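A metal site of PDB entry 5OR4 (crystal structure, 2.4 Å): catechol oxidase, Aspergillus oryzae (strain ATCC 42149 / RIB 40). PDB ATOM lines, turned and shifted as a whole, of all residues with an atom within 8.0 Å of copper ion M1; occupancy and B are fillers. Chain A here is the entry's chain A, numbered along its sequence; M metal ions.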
ATOM      1  N   HIS A 102     -33.868  -0.031   8.989  1.00  0.00           N
ATOM      2  CA  HIS A 102     -32.414  -0.127   8.987  1.00  0.00           C
ATOM      3  C   HIS A 102     -31.803   0.827   7.963  1.00  0.00           C
ATOM      4  O   HIS A 102     -30.808   1.495   8.251  1.00  0.00           O
ATOM      5  CB  HIS A 102     -31.981  -1.569   8.698  1.00  0.00           C
ATOM      6  CG  HIS A 102     -30.528  -1.825   8.930  1.00  0.00           C
ATOM      7  ND1 HIS A 102     -29.576  -1.697   7.937  1.00  0.00           N
ATOM      8  CD2 HIS A 102     -29.843  -2.204  10.046  1.00  0.00           C
ATOM      9  CE1 HIS A 102     -28.383  -1.984   8.423  1.00  0.00           C
ATOM     10  NE2 HIS A 102     -28.520  -2.291   9.703  1.00  0.00           N
ATOM     11  N   HIS A 110     -24.356   2.761  13.148  1.00  0.00           N
ATOM     12  CA  HIS A 110     -23.053   2.157  12.884  1.00  0.00           C
ATOM     13  C   HIS A 110     -21.962   3.153  13.232  1.00  0.00           C
ATOM     14  O   HIS A 110     -22.055   4.327  12.882  1.00  0.00           O
ATOM     15  CB  HIS A 110     -22.931   1.703  11.420  1.00  0.00           C
ATOM     16  CG  HIS A 110     -23.974   0.703  11.009  1.00  0.00           C
ATOM     17  ND1 HIS A 110     -25.069   1.055  10.248  1.00  0.00           N
ATOM     18  CD2 HIS A 110     -24.086  -0.619  11.236  1.00  0.00           C
ATOM     19  CE1 HIS A 110     -25.815  -0.013  10.041  1.00  0.00           C
ATOM     20  NE2 HIS A 110     -25.237  -1.051  10.627  1.00  0.00           N
ATOM     21  N   PHE A 115     -24.409   1.250  18.580  1.00  0.00           N
ATOM     22  CA  PHE A 115     -24.279   0.214  17.570  1.00  0.00           C
ATOM     23  C   PHE A 115     -24.595  -1.171  18.122  1.00  0.00           C
ATOM     24  O   PHE A 115     -25.420  -1.905  17.567  1.00  0.00           O
ATOM     25  CB  PHE A 115     -22.871   0.232  16.964  1.00  0.00           C
ATOM     26  CG  PHE A 115     -22.521  -1.028  16.226  1.00  0.00           C
ATOM     27  CD1 PHE A 115     -23.163  -1.360  15.045  1.00  0.00           C
ATOM     28  CD2 PHE A 115     -21.545  -1.891  16.717  1.00  0.00           C
ATOM     29  CE1 PHE A 115     -22.846  -2.524  14.369  1.00  0.00           C
ATOM     30  CE2 PHE A 115     -21.225  -3.046  16.039  1.00  0.00           C
ATOM     31  CZ  PHE A 115     -21.871  -3.364  14.862  1.00  0.00           C
ATOM     32  N   HIS A 119     -28.537  -3.198  17.680  1.00  0.00           N
ATOM     33  CA  HIS A 119     -28.691  -4.456  16.960  1.00  0.00           C
ATOM     34  C   HIS A 119     -29.142  -5.580  17.878  1.00  0.00           C
ATOM     35  O   HIS A 119     -29.830  -6.501  17.414  1.00  0.00           O
ATOM     36  CB  HIS A 119     -27.379  -4.813  16.267  1.00  0.00           C
ATOM     37  CG  HIS A 119     -27.084  -3.974  15.061  1.00  0.00           C
ATOM     38  ND1 HIS A 119     -26.447  -2.755  15.146  1.00  0.00           N
ATOM     39  CD2 HIS A 119     -27.366  -4.164  13.749  1.00  0.00           C
ATOM     40  CE1 HIS A 119     -26.337  -2.236  13.932  1.00  0.00           C
ATOM     41  NE2 HIS A 119     -26.884  -3.072  13.067  1.00  0.00           N
ATOM     42  N   GLN A 273     -15.891  -3.654  14.357  1.00  0.00           N
ATOM     43  CA  GLN A 273     -16.380  -3.096  13.104  1.00  0.00           C
ATOM     44  C   GLN A 273     -15.288  -2.806  12.099  1.00  0.00           C
ATOM     45  O   GLN A 273     -15.573  -2.724  10.889  1.00  0.00           O
ATOM     46  CB  GLN A 273     -17.165  -1.810  13.367  1.00  0.00           C
ATOM     47  CG  GLN A 273     -18.412  -2.002  14.215  1.00  0.00           C
ATOM     48  CD  GLN A 273     -19.035  -0.678  14.630  1.00  0.00           C
ATOM     49  OE1 GLN A 273     -19.833  -0.097  13.897  1.00  0.00           O
ATOM     50  NE2 GLN A 273     -18.665  -0.205  15.818  1.00  0.00           N
ATOM     51  N   VAL A 283     -14.542  -8.519  12.518  1.00  0.00           N
ATOM     52  CA  VAL A 283     -15.384  -9.691  12.313  1.00  0.00           C
ATOM     53  C   VAL A 283     -16.755  -9.277  11.813  1.00  0.00           C
ATOM     54  O   VAL A 283     -17.408 -10.034  11.085  1.00  0.00           O
ATOM     55  CB  VAL A 283     -15.485 -10.511  13.616  1.00  0.00           C
ATOM     56  CG1 VAL A 283     -14.124 -11.042  14.021  1.00  0.00           C
ATOM     57  CG2 VAL A 283     -16.096  -9.683  14.732  1.00  0.00           C
ATOM     58  N   HIS A 284     -17.216  -8.074  12.170  1.00  0.00           N
ATOM     59  CA  HIS A 284     -18.517  -7.605  11.702  1.00  0.00           C
ATOM     60  C   HIS A 284     -18.487  -7.357  10.191  1.00  0.00           C
ATOM     61  O   HIS A 284     -19.374  -7.816   9.459  1.00  0.00           O
ATOM     62  CB  HIS A 284     -18.921  -6.336  12.449  1.00  0.00           C
ATOM     63  CG  HIS A 284     -20.201  -5.728  11.955  1.00  0.00           C
ATOM     64  ND1 HIS A 284     -20.242  -4.507  11.311  1.00  0.00           N
ATOM     65  CD2 HIS A 284     -21.482  -6.169  12.015  1.00  0.00           C
ATOM     66  CE1 HIS A 284     -21.491  -4.230  10.985  1.00  0.00           C
ATOM     67  NE2 HIS A 284     -22.267  -5.221  11.405  1.00  0.00           N
ATOM     68  N   GLY A 285     -17.487  -6.628   9.713  1.00  0.00           N
ATOM     69  CA  GLY A 285     -17.364  -6.401   8.285  1.00  0.00           C
ATOM     70  C   GLY A 285     -17.062  -7.670   7.517  1.00  0.00           C
ATOM     71  O   GLY A 285     -17.556  -7.883   6.409  1.00  0.00           O
ATOM     72  N   GLY A 287     -18.030 -10.698   8.207  1.00  0.00           N
ATOM     73  CA  GLY A 287     -19.218 -11.529   8.091  1.00  0.00           C
ATOM     74  C   GLY A 287     -20.181 -11.030   7.031  1.00  0.00           C
ATOM     75  O   GLY A 287     -20.832 -11.814   6.346  1.00  0.00           O
ATOM     76  N   HIS A 288     -20.291  -9.702   6.888  1.00  0.00           N
ATOM     77  CA  HIS A 288     -21.217  -9.142   5.904  1.00  0.00           C
ATOM     78  C   HIS A 288     -20.727  -9.369   4.483  1.00  0.00           C
ATOM     79  O   HIS A 288     -21.476  -9.862   3.633  1.00  0.00           O
ATOM     80  CB  HIS A 288     -21.408  -7.643   6.158  1.00  0.00           C
ATOM     81  CG  HIS A 288     -22.399  -7.336   7.240  1.00  0.00           C
ATOM     82  ND1 HIS A 288     -23.762  -7.398   7.038  1.00  0.00           N
ATOM     83  CD2 HIS A 288     -22.227  -6.960   8.526  1.00  0.00           C
ATOM     84  CE1 HIS A 288     -24.381  -7.071   8.158  1.00  0.00           C
ATOM     85  NE2 HIS A 288     -23.479  -6.806   9.076  1.00  0.00           N
ATOM     86  N   MET A 291     -20.580 -12.836   2.254  1.00  0.00           N
ATOM     87  CA  MET A 291     -21.730 -13.291   1.480  1.00  0.00           C
ATOM     88  C   MET A 291     -21.692 -12.789   0.041  1.00  0.00           C
ATOM     89  O   MET A 291     -22.142 -13.484  -0.872  1.00  0.00           O
ATOM     90  CB  MET A 291     -23.035 -12.845   2.140  1.00  0.00           C
ATOM     91  CG  MET A 291     -23.111 -13.099   3.643  1.00  0.00           C
ATOM     92  SD  MET A 291     -24.655 -12.454   4.341  1.00  0.00           S
ATOM     93  CE  MET A 291     -24.179 -12.203   6.044  1.00  0.00           C
ATOM     94  N   VAL A 299     -24.323  -1.486   2.955  1.00  0.00           N
ATOM     95  CA  VAL A 299     -24.310  -1.256   4.394  1.00  0.00           C
ATOM     96  C   VAL A 299     -25.711  -0.916   4.894  1.00  0.00           C
ATOM     97  O   VAL A 299     -26.074  -1.256   6.036  1.00  0.00           O
ATOM     98  CB  VAL A 299     -23.289  -0.150   4.732  1.00  0.00           C
ATOM     99  CG1 VAL A 299     -23.507   0.404   6.132  1.00  0.00           C
ATOM    100  CG2 VAL A 299     -21.871  -0.684   4.581  1.00  0.00           C
ATOM    101  N   SER A 302     -28.357  -4.289   4.163  1.00  0.00           N
ATOM    102  CA  SER A 302     -27.827  -5.611   4.512  1.00  0.00           C
ATOM    103  C   SER A 302     -28.815  -6.538   5.213  1.00  0.00           C
ATOM    104  O   SER A 302     -28.709  -7.766   4.993  1.00  0.00           O
ATOM    105  CB  SER A 302     -26.558  -5.455   5.369  1.00  0.00           C
ATOM    106  OG  SER A 302     -26.813  -4.764   6.569  1.00  0.00           O
ATOM    107  N   PRO A 303     -29.779  -6.086   6.033  1.00  0.00           N
ATOM    108  CA  PRO A 303     -30.789  -7.019   6.561  1.00  0.00           C
ATOM    109  C   PRO A 303     -31.611  -7.700   5.485  1.00  0.00           C
ATOM    110  O   PRO A 303     -32.305  -8.683   5.788  1.00  0.00           O
ATOM    111  CB  PRO A 303     -31.662  -6.128   7.453  1.00  0.00           C
ATOM    112  CG  PRO A 303     -30.754  -5.055   7.878  1.00  0.00           C
ATOM    113  CD  PRO A 303     -29.886  -4.764   6.691  1.00  0.00           C
ATOM    114  N   PHE A 308     -28.386 -12.282   7.642  1.00  0.00           N
ATOM    115  CA  PHE A 308     -28.104 -11.156   8.521  1.00  0.00           C
ATOM    116  C   PHE A 308     -28.435 -11.486   9.971  1.00  0.00           C
ATOM    117  O   PHE A 308     -27.679 -11.125  10.889  1.00  0.00           O
ATOM    118  CB  PHE A 308     -28.892  -9.929   8.049  1.00  0.00           C
ATOM    119  CG  PHE A 308     -28.876  -8.761   8.996  1.00  0.00           C
ATOM    120  CD1 PHE A 308     -29.828  -8.642   9.994  1.00  0.00           C
ATOM    121  CD2 PHE A 308     -27.936  -7.759   8.852  1.00  0.00           C
ATOM    122  CE1 PHE A 308     -29.814  -7.569  10.865  1.00  0.00           C
ATOM    123  CE2 PHE A 308     -27.924  -6.677   9.713  1.00  0.00           C
ATOM    124  CZ  PHE A 308     -28.862  -6.583  10.713  1.00  0.00           C
ATOM    125  N   HIS A 311     -26.044 -13.858  11.440  1.00  0.00           N
ATOM    126  CA  HIS A 311     -24.786 -13.137  11.565  1.00  0.00           C
ATOM    127  C   HIS A 311     -24.774 -12.269  12.806  1.00  0.00           C
ATOM    128  O   HIS A 311     -23.780 -12.234  13.549  1.00  0.00           O
ATOM    129  CB  HIS A 311     -24.545 -12.296  10.310  1.00  0.00           C
ATOM    130  CG  HIS A 311     -23.372 -11.374  10.418  1.00  0.00           C
ATOM    131  ND1 HIS A 311     -22.131 -11.793  10.855  1.00  0.00           N
ATOM    132  CD2 HIS A 311     -23.238 -10.058  10.131  1.00  0.00           C
ATOM    133  CE1 HIS A 311     -21.293 -10.778  10.842  1.00  0.00           C
ATOM    134  NE2 HIS A 311     -21.935  -9.706  10.413  1.00  0.00           N
ATOM    135  N   HIS A 312     -25.874 -11.555  13.074  1.00  0.00           N
ATOM    136  CA  HIS A 312     -25.921 -10.668  14.223  1.00  0.00           C
ATOM    137  C   HIS A 312     -26.294 -11.381  15.519  1.00  0.00           C
ATOM    138  O   HIS A 312     -26.166 -10.783  16.591  1.00  0.00           O
ATOM    139  CB  HIS A 312     -26.901  -9.527  13.951  1.00  0.00           C
ATOM    140  CG  HIS A 312     -26.239  -8.297  13.418  1.00  0.00           C
ATOM    141  ND1 HIS A 312     -25.571  -7.407  14.216  1.00  0.00           N
ATOM    142  CD2 HIS A 312     -26.127  -7.840  12.152  1.00  0.00           C
ATOM    143  CE1 HIS A 312     -25.072  -6.438  13.468  1.00  0.00           C
ATOM    144  NE2 HIS A 312     -25.399  -6.668  12.214  1.00  0.00           N
ATOM    145  N   ILE A 315     -22.671 -11.743  16.524  1.00  0.00           N
ATOM    146  CA  ILE A 315     -22.166 -10.447  16.970  1.00  0.00           C
ATOM    147  C   ILE A 315     -22.608 -10.182  18.400  1.00  0.00           C
ATOM    148  O   ILE A 315     -21.814  -9.759  19.253  1.00  0.00           O
ATOM    149  CB  ILE A 315     -22.631  -9.329  16.022  1.00  0.00           C
ATOM    150  CG1 ILE A 315     -21.878  -9.403  14.690  1.00  0.00           C
ATOM    151  CG2 ILE A 315     -22.439  -7.958  16.658  1.00  0.00           C
ATOM    152  CD1 ILE A 315     -20.410  -9.092  14.802  1.00  0.00           C
HETATM  153 CU    CU M   1     -24.084  -6.022  10.801  1.00  0.00          CU
HETATM  154 CU    CU M   2     -26.965  -2.318  11.134  1.00  0.00          CU
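O of His 284 lies within hydrogen-bond range of NE2 of His 311, 3.3 Å away.
Along chain A the residues within 4 Å of copper ion M1 span positions 284 to 312.
Copper ion M1 is bound by NE2 of His 288 (2.0 Å), NE2 of His 312 (2.0 Å) and NE2 of His 284 (2.1 Å).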
